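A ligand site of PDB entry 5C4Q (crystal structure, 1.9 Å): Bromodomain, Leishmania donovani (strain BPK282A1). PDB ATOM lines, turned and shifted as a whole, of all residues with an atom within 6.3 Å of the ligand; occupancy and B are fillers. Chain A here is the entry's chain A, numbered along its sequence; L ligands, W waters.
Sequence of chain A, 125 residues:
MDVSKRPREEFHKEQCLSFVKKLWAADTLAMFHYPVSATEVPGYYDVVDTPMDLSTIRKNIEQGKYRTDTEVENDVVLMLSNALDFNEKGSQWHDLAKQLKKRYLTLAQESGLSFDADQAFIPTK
O of Met 31 lies close to O1 of the ligand, 3.0 Å away. Merely in contact with the ligand: Phe 86, His 33, Val 41, Glu 40, Val 36, Tyr 44 and Pro 35. Hydrophobic or aromatic side chains within 4 Å of the ligand: Met 31, His 33, Tyr 34, Val 36, Val 41, Tyr 44, Phe 86 and Trp 93. Within 4 Å of the ligand: Ala 30, Met 31, His 33, Tyr 34, Pro 35, Val 36, Glu 40, Val 41, Tyr 44, Phe 86, Asn 87 and Trp 93. The nearest printed residue that does not touch the ligand is Ala 83 (4.1 Å).
The backbone NH of Met 31 lies within hydrogen-bond range of the side-chain carboxylate of Asp 27, 2.9 Å away. The side-chain amide nitrogen of Asn 87 sits at hydrogen-bond distance from the backbone carbonyl oxygen of Ala 83. N of Ala 30 lies within hydrogen-bond range of OD1 of Asp 27 (2.9 Å).
Water W4 lies within hydrogen-bond range of the side-chain hydroxyl (OH) of Tyr 44, a nitrogen (N6) of the ligand, the backbone NH (N) of Ala 83 and the backbone carbonyl oxygen (O) of Asn 82. Water W2 bridges OE2 of Glu 40 and N of Ser 37. Water W5 lies within hydrogen-bond range of a nitrogen (N2) of the ligand and the backbone carbonyl oxygen (O) of Ala 30.
NE1 of Trp 93 sits close to O3 of the ligand. The backbone NH (N) of Tyr 34 is in hydrogen-bond range of an oxygen (O2) of the ligand (2.9 Å). O of Ala 30 is in hydrogen-bond range of N2 of the ligand (3.0 Å). ND2 of Asn 87 sits at hydrogen-bond distance from N5 of the ligand (2.8 Å).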
ATOM      1  N   ASP A  27     -10.473   5.293 -23.307  1.00  0.00           N
ATOM      2  CA  ASP A  27      -9.775   4.640 -22.214  1.00  0.00           C
ATOM      3  C   ASP A  27      -8.369   4.293 -22.657  1.00  0.00           C
ATOM      4  O   ASP A  27      -8.111   3.187 -23.133  1.00  0.00           O
ATOM      5  CB  ASP A  27     -10.547   3.398 -21.785  1.00  0.00           C
ATOM      6  CG  ASP A  27      -9.866   2.602 -20.701  1.00  0.00           C
ATOM      7  OD1 ASP A  27      -8.757   2.977 -20.237  1.00  0.00           O
ATOM      8  OD2 ASP A  27     -10.462   1.582 -20.320  1.00  0.00           O
ATOM      9  N   LEU A  29      -5.660   3.607 -21.168  1.00  0.00           N
ATOM     10  CA  LEU A  29      -4.910   2.617 -20.421  1.00  0.00           C
ATOM     11  C   LEU A  29      -5.562   1.237 -20.459  1.00  0.00           C
ATOM     12  O   LEU A  29      -5.038   0.297 -19.878  1.00  0.00           O
ATOM     13  CB  LEU A  29      -4.754   3.056 -18.968  1.00  0.00           C
ATOM     14  CG  LEU A  29      -4.056   4.383 -18.695  1.00  0.00           C
ATOM     15  CD1 LEU A  29      -3.961   4.651 -17.185  1.00  0.00           C
ATOM     16  CD2 LEU A  29      -2.689   4.348 -19.330  1.00  0.00           C
ATOM     17  N   ALA A  30      -6.710   1.143 -21.136  1.00  0.00           N
ATOM     18  CA  ALA A  30      -7.531  -0.070 -21.116  1.00  0.00           C
ATOM     19  C   ALA A  30      -7.893  -0.464 -19.683  1.00  0.00           C
ATOM     20  O   ALA A  30      -8.043  -1.652 -19.373  1.00  0.00           O
ATOM     21  CB  ALA A  30      -6.821  -1.230 -21.818  1.00  0.00           C
ATOM     22  N   MET A  31      -8.042   0.525 -18.814  1.00  0.00           N
ATOM     23  CA  MET A  31      -8.226   0.183 -17.411  1.00  0.00           C
ATOM     24  C   MET A  31      -9.679  -0.179 -17.114  1.00  0.00           C
ATOM     25  O   MET A  31      -9.953  -0.920 -16.170  1.00  0.00           O
ATOM     26  CB  MET A  31      -7.776   1.338 -16.501  1.00  0.00           C
ATOM     27  CG  MET A  31      -8.571   2.629 -16.623  1.00  0.00           C
ATOM     28  SD  MET A  31      -7.910   3.917 -15.542  1.00  0.00           S
ATOM     29  CE  MET A  31      -8.394   3.295 -13.927  1.00  0.00           C
ATOM     30  N   PHE A  32     -10.594   0.323 -17.920  1.00  0.00           N
ATOM     31  CA  PHE A  32     -12.019   0.154 -17.648  1.00  0.00           C
ATOM     32  C   PHE A  32     -12.661  -0.961 -18.470  1.00  0.00           C
ATOM     33  O   PHE A  32     -13.869  -1.186 -18.393  1.00  0.00           O
ATOM     34  CB  PHE A  32     -12.751   1.470 -17.917  1.00  0.00           C
ATOM     35  CG  PHE A  32     -12.334   2.603 -17.029  1.00  0.00           C
ATOM     36  CD1 PHE A  32     -12.563   2.552 -15.649  1.00  0.00           C
ATOM     37  CD2 PHE A  32     -11.778   3.760 -17.568  1.00  0.00           C
ATOM     38  CE1 PHE A  32     -12.207   3.619 -14.832  1.00  0.00           C
ATOM     39  CE2 PHE A  32     -11.422   4.827 -16.751  1.00  0.00           C
ATOM     40  CZ  PHE A  32     -11.641   4.767 -15.385  1.00  0.00           C
ATOM     41  N   HIS A  33     -11.859  -1.652 -19.270  1.00  0.00           N
ATOM     42  CA  HIS A  33     -12.385  -2.592 -20.247  1.00  0.00           C
ATOM     43  C   HIS A  33     -13.034  -3.872 -19.660  1.00  0.00           C
ATOM     44  O   HIS A  33     -14.039  -4.334 -20.192  1.00  0.00           O
ATOM     45  CB  HIS A  33     -11.278  -2.973 -21.232  1.00  0.00           C
ATOM     46  CG  HIS A  33     -10.965  -1.899 -22.233  1.00  0.00           C
ATOM     47  ND1 HIS A  33     -10.093  -2.075 -23.279  1.00  0.00           N
ATOM     48  CD2 HIS A  33     -11.427  -0.627 -22.348  1.00  0.00           C
ATOM     49  CE1 HIS A  33     -10.029  -0.969 -23.999  1.00  0.00           C
ATOM     50  NE2 HIS A  33     -10.832  -0.076 -23.448  1.00  0.00           N
ATOM     51  N   TYR A  34     -12.469  -4.419 -18.584  1.00  0.00           N
ATOM     52  CA  TYR A  34     -12.952  -5.674 -17.993  1.00  0.00           C
ATOM     53  C   TYR A  34     -13.048  -5.556 -16.487  1.00  0.00           C
ATOM     54  O   TYR A  34     -12.393  -4.692 -15.900  1.00  0.00           O
ATOM     55  CB  TYR A  34     -12.019  -6.851 -18.362  1.00  0.00           C
ATOM     56  CG  TYR A  34     -11.836  -6.924 -19.836  1.00  0.00           C
ATOM     57  CD1 TYR A  34     -12.855  -7.372 -20.652  1.00  0.00           C
ATOM     58  CD2 TYR A  34     -10.663  -6.484 -20.433  1.00  0.00           C
ATOM     59  CE1 TYR A  34     -12.710  -7.402 -22.015  1.00  0.00           C
ATOM     60  CE2 TYR A  34     -10.500  -6.523 -21.806  1.00  0.00           C
ATOM     61  CZ  TYR A  34     -11.530  -6.976 -22.586  1.00  0.00           C
ATOM     62  OH  TYR A  34     -11.404  -6.993 -23.957  1.00  0.00           O
ATOM     63  N   PRO A  35     -13.849  -6.428 -15.835  1.00  0.00           N
ATOM     64  CA  PRO A  35     -13.798  -6.486 -14.369  1.00  0.00           C
ATOM     65  C   PRO A  35     -12.355  -6.662 -13.899  1.00  0.00           C
ATOM     66  O   PRO A  35     -11.571  -7.330 -14.565  1.00  0.00           O
ATOM     67  CB  PRO A  35     -14.641  -7.706 -14.014  1.00  0.00           C
ATOM     68  CG  PRO A  35     -15.509  -7.939 -15.196  1.00  0.00           C
ATOM     69  CD  PRO A  35     -14.783  -7.420 -16.402  1.00  0.00           C
ATOM     70  N   VAL A  36     -11.994  -6.008 -12.804  1.00  0.00           N
ATOM     71  CA  VAL A  36     -10.634  -6.056 -12.317  1.00  0.00           C
ATOM     72  C   VAL A  36     -10.269  -7.452 -11.824  1.00  0.00           C
ATOM     73  O   VAL A  36     -11.048  -8.056 -11.096  1.00  0.00           O
ATOM     74  CB  VAL A  36     -10.428  -5.037 -11.187  1.00  0.00           C
ATOM     75  CG1 VAL A  36      -9.180  -5.370 -10.374  1.00  0.00           C
ATOM     76  CG2 VAL A  36     -10.348  -3.638 -11.770  1.00  0.00           C
ATOM     77  N   SER A  37      -9.117  -7.968 -12.249  1.00  0.00           N
ATOM     78  CA  SER A  37      -8.586  -9.194 -11.660  1.00  0.00           C
ATOM     79  C   SER A  37      -7.744  -8.850 -10.439  1.00  0.00           C
ATOM     80  O   SER A  37      -6.754  -8.108 -10.530  1.00  0.00           O
ATOM     81  CB  SER A  37      -7.743  -9.989 -12.667  1.00  0.00           C
ATOM     82  OG  SER A  37      -8.561 -10.669 -13.601  1.00  0.00           O
ATOM     83  N   GLU A  40      -4.085  -8.878 -10.578  1.00  0.00           N
ATOM     84  CA  GLU A  40      -3.412  -7.818 -11.343  1.00  0.00           C
ATOM     85  C   GLU A  40      -3.484  -6.482 -10.606  1.00  0.00           C
ATOM     86  O   GLU A  40      -2.631  -5.610 -10.797  1.00  0.00           O
ATOM     87  CB  GLU A  40      -4.018  -7.691 -12.754  1.00  0.00           C
ATOM     88  CG  GLU A  40      -3.867  -8.966 -13.592  1.00  0.00           C
ATOM     89  CD  GLU A  40      -4.715  -8.983 -14.857  1.00  0.00           C
ATOM     90  OE1 GLU A  40      -4.644 -10.002 -15.575  1.00  0.00           O
ATOM     91  OE2 GLU A  40      -5.451  -8.006 -15.122  1.00  0.00           O
ATOM     92  N   VAL A  41      -4.508  -6.330  -9.781  1.00  0.00           N
ATOM     93  CA  VAL A  41      -4.658  -5.144  -8.945  1.00  0.00           C
ATOM     94  C   VAL A  41      -4.934  -5.613  -7.532  1.00  0.00           C
ATOM     95  O   VAL A  41      -6.092  -5.701  -7.100  1.00  0.00           O
ATOM     96  CB  VAL A  41      -5.799  -4.222  -9.450  1.00  0.00           C
ATOM     97  CG1 VAL A  41      -5.755  -2.898  -8.723  1.00  0.00           C
ATOM     98  CG2 VAL A  41      -5.690  -4.000 -10.956  1.00  0.00           C
ATOM     99  N   PRO A  42      -3.874  -5.959  -6.796  1.00  0.00           N
ATOM    100  CA  PRO A  42      -4.062  -6.515  -5.461  1.00  0.00           C
ATOM    101  C   PRO A  42      -4.775  -5.538  -4.523  1.00  0.00           C
ATOM    102  O   PRO A  42      -4.513  -4.332  -4.515  1.00  0.00           O
ATOM    103  CB  PRO A  42      -2.639  -6.798  -4.997  1.00  0.00           C
ATOM    104  CG  PRO A  42      -1.890  -7.020  -6.273  1.00  0.00           C
ATOM    105  CD  PRO A  42      -2.454  -5.998  -7.207  1.00  0.00           C
ATOM    106  N   TYR A  44      -7.820  -4.670  -4.704  1.00  0.00           N
ATOM    107  CA  TYR A  44      -8.835  -3.859  -5.380  1.00  0.00           C
ATOM    108  C   TYR A  44     -10.220  -4.003  -4.736  1.00  0.00           C
ATOM    109  O   TYR A  44     -10.864  -3.001  -4.420  1.00  0.00           O
ATOM    110  CB  TYR A  44      -8.925  -4.212  -6.878  1.00  0.00           C
ATOM    111  CG  TYR A  44      -9.897  -3.319  -7.599  1.00  0.00           C
ATOM    112  CD1 TYR A  44      -9.540  -2.037  -7.983  1.00  0.00           C
ATOM    113  CD2 TYR A  44     -11.194  -3.740  -7.857  1.00  0.00           C
ATOM    114  CE1 TYR A  44     -10.444  -1.199  -8.627  1.00  0.00           C
ATOM    115  CE2 TYR A  44     -12.099  -2.933  -8.498  1.00  0.00           C
ATOM    116  CZ  TYR A  44     -11.732  -1.665  -8.880  1.00  0.00           C
ATOM    117  OH  TYR A  44     -12.650  -0.858  -9.503  1.00  0.00           O
ATOM    118  N   MET A  52     -17.723  -1.970 -11.422  1.00  0.00           N
ATOM    119  CA  MET A  52     -18.406  -1.752 -12.683  1.00  0.00           C
ATOM    120  C   MET A  52     -17.327  -1.564 -13.732  1.00  0.00           C
ATOM    121  O   MET A  52     -16.274  -1.003 -13.451  1.00  0.00           O
ATOM    122  CB  MET A  52     -19.349  -0.538 -12.622  1.00  0.00           C
ATOM    123  CG  MET A  52     -20.155  -0.327 -13.896  1.00  0.00           C
ATOM    124  SD  MET A  52     -21.064  -1.803 -14.411  1.00  0.00           S
ATOM    125  CE  MET A  52     -22.064  -2.079 -12.941  1.00  0.00           C
ATOM    126  N   MET A  79     -18.567   3.526 -12.306  1.00  0.00           N
ATOM    127  CA  MET A  79     -17.301   3.008 -12.774  1.00  0.00           C
ATOM    128  C   MET A  79     -16.179   4.023 -12.559  1.00  0.00           C
ATOM    129  O   MET A  79     -15.125   3.685 -12.032  1.00  0.00           O
ATOM    130  CB  MET A  79     -17.401   2.641 -14.258  1.00  0.00           C
ATOM    131  CG  MET A  79     -16.099   2.108 -14.852  1.00  0.00           C
ATOM    132  SD  MET A  79     -16.290   1.894 -16.630  1.00  0.00           S
ATOM    133  CE  MET A  79     -16.071   3.597 -17.186  1.00  0.00           C
ATOM    134  N   ASN A  82     -15.358   4.667  -8.778  1.00  0.00           N
ATOM    135  CA  ASN A  82     -14.525   3.619  -8.208  1.00  0.00           C
ATOM    136  C   ASN A  82     -13.042   3.868  -8.461  1.00  0.00           C
ATOM    137  O   ASN A  82     -12.212   3.651  -7.580  1.00  0.00           O
ATOM    138  CB  ASN A  82     -14.921   2.243  -8.770  1.00  0.00           C
ATOM    139  CG  ASN A  82     -16.296   1.798  -8.320  1.00  0.00           C
ATOM    140  OD1 ASN A  82     -16.871   2.369  -7.392  1.00  0.00           O
ATOM    141  ND2 ASN A  82     -16.840   0.776  -8.983  1.00  0.00           N
ATOM    142  N   ALA A  83     -12.721   4.316  -9.672  1.00  0.00           N
ATOM    143  CA  ALA A  83     -11.335   4.553 -10.049  1.00  0.00           C
ATOM    144  C   ALA A  83     -10.775   5.748  -9.302  1.00  0.00           C
ATOM    145  O   ALA A  83      -9.613   5.754  -8.898  1.00  0.00           O
ATOM    146  CB  ALA A  83     -11.216   4.767 -11.570  1.00  0.00           C
ATOM    147  N   PHE A  86     -10.288   4.417  -5.566  1.00  0.00           N
ATOM    148  CA  PHE A  86      -9.220   3.433  -5.381  1.00  0.00           C
ATOM    149  C   PHE A  86      -7.844   4.056  -5.599  1.00  0.00           C
ATOM    150  O   PHE A  86      -6.911   3.780  -4.855  1.00  0.00           O
ATOM    151  CB  PHE A  86      -9.399   2.249  -6.319  1.00  0.00           C
ATOM    152  CG  PHE A  86      -8.318   1.199  -6.209  1.00  0.00           C
ATOM    153  CD1 PHE A  86      -8.304   0.303  -5.156  1.00  0.00           C
ATOM    154  CD2 PHE A  86      -7.323   1.113  -7.170  1.00  0.00           C
ATOM    155  CE1 PHE A  86      -7.317  -0.676  -5.068  1.00  0.00           C
ATOM    156  CE2 PHE A  86      -6.328   0.138  -7.093  1.00  0.00           C
ATOM    157  CZ  PHE A  86      -6.323  -0.758  -6.046  1.00  0.00           C
ATOM    158  N   ASN A  87      -7.723   4.895  -6.621  1.00  0.00           N
ATOM    159  CA  ASN A  87      -6.413   5.352  -7.027  1.00  0.00           C
ATOM    160  C   ASN A  87      -5.958   6.619  -6.338  1.00  0.00           C
ATOM    161  O   ASN A  87      -6.761   7.406  -5.859  1.00  0.00           O
ATOM    162  CB  ASN A  87      -6.371   5.533  -8.541  1.00  0.00           C
ATOM    163  CG  ASN A  87      -6.541   4.239  -9.277  1.00  0.00           C
ATOM    164  OD1 ASN A  87      -5.625   3.396  -9.315  1.00  0.00           O
ATOM    165  ND2 ASN A  87      -7.722   4.040  -9.850  1.00  0.00           N
ATOM    166  N   SER A  91      -1.780   9.738 -10.093  1.00  0.00           N
ATOM    167  CA  SER A  91      -1.457   8.475 -10.755  1.00  0.00           C
ATOM    168  C   SER A  91      -2.092   8.454 -12.142  1.00  0.00           C
ATOM    169  O   SER A  91      -3.106   9.109 -12.370  1.00  0.00           O
ATOM    170  CB  SER A  91      -1.930   7.287  -9.929  1.00  0.00           C
ATOM    171  OG  SER A  91      -3.336   7.304  -9.791  1.00  0.00           O
ATOM    172  N   TRP A  93      -3.730   6.202 -13.491  1.00  0.00           N
ATOM    173  CA  TRP A  93      -5.072   5.638 -13.325  1.00  0.00           C
ATOM    174  C   TRP A  93      -6.098   6.715 -12.907  1.00  0.00           C
ATOM    175  O   TRP A  93      -7.157   6.844 -13.519  1.00  0.00           O
ATOM    176  CB  TRP A  93      -5.045   4.510 -12.291  1.00  0.00           C
ATOM    177  CG  TRP A  93      -3.935   3.524 -12.476  1.00  0.00           C
ATOM    178  CD1 TRP A  93      -2.817   3.410 -11.701  1.00  0.00           C
ATOM    179  CD2 TRP A  93      -3.835   2.515 -13.487  1.00  0.00           C
ATOM    180  NE1 TRP A  93      -2.022   2.385 -12.170  1.00  0.00           N
ATOM    181  CE2 TRP A  93      -2.623   1.827 -13.267  1.00  0.00           C
ATOM    182  CE3 TRP A  93      -4.643   2.119 -14.563  1.00  0.00           C
ATOM    183  CZ2 TRP A  93      -2.202   0.769 -14.074  1.00  0.00           C
ATOM    184  CZ3 TRP A  93      -4.220   1.071 -15.374  1.00  0.00           C
ATOM    185  CH2 TRP A  93      -3.009   0.408 -15.116  1.00  0.00           C
HETATM  186  C1  LIG L   1      -5.777  -2.326 -14.338  1.00  0.00           C
HETATM  187  N1  LIG L   1      -7.482  -1.024 -13.267  1.00  0.00           N
HETATM  188  C2  LIG L   1      -5.698   0.245 -11.420  1.00  0.00           C
HETATM  189  C3  LIG L   1      -3.596   0.297 -10.065  1.00  0.00           C
HETATM  190  C4  LIG L   1      -5.267  -0.671 -12.367  1.00  0.00           C
HETATM  191  C5  LIG L   1     -10.288  -0.179 -12.980  1.00  0.00           C
HETATM  192  C6  LIG L   1      -4.216  -3.950 -15.283  1.00  0.00           C
HETATM  193  C7  LIG L   1      -4.671  -5.289 -17.371  1.00  0.00           C
HETATM  194  C8  LIG L   1      -5.089  -4.271 -16.353  1.00  0.00           C
HETATM  195  C9  LIG L   1      -6.311  -3.599 -16.396  1.00  0.00           C
HETATM  196  N2  LIG L   1      -7.264  -3.872 -17.453  1.00  0.00           N
HETATM  197  S1  LIG L   1      -8.819  -4.431 -17.166  1.00  0.00           S
HETATM  198  C10 LIG L   1      -8.693  -6.091 -16.856  1.00  0.00           C
HETATM  199  O1  LIG L   1      -9.242  -3.792 -15.962  1.00  0.00           O
HETATM  200  O2  LIG L   1      -9.593  -4.234 -18.344  1.00  0.00           O
HETATM  201  C11 LIG L   1      -6.635  -2.656 -15.392  1.00  0.00           C
HETATM  202  C12 LIG L   1      -6.172  -1.317 -13.300  1.00  0.00           C
HETATM  203  N3  LIG L   1      -7.870  -0.111 -12.329  1.00  0.00           N
HETATM  204  C13 LIG L   1      -7.057   0.551 -11.387  1.00  0.00           C
HETATM  205  N4  LIG L   1      -4.829   0.903 -10.452  1.00  0.00           N
HETATM  206  O3  LIG L   1      -2.960   1.105  -9.126  1.00  0.00           O
HETATM  207  O4  LIG L   1      -3.173  -0.719 -10.482  1.00  0.00           O
HETATM  208  N5  LIG L   1      -7.877   1.361 -10.666  1.00  0.00           N
HETATM  209  N6  LIG L   1      -9.141   1.221 -11.116  1.00  0.00           N
HETATM  210  C14 LIG L   1      -9.175   0.318 -12.143  1.00  0.00           C
HETATM  211  C15 LIG L   1      -4.554  -2.998 -14.294  1.00  0.00           C
HETATM  212  O   HOH W   1     -13.625  -0.609 -13.789  1.00  0.00           O
HETATM  213  O   HOH W   2      -7.533  -6.569 -14.100  1.00  0.00           O
HETATM  214  O   HOH W   3     -12.043  -2.147 -14.982  1.00  0.00           O
HETATM  215  O   HOH W   4     -11.555   1.407 -10.124  1.00  0.00           O
HETATM  216  O   HOH W   5      -7.084  -4.503 -20.610  1.00  0.00           O
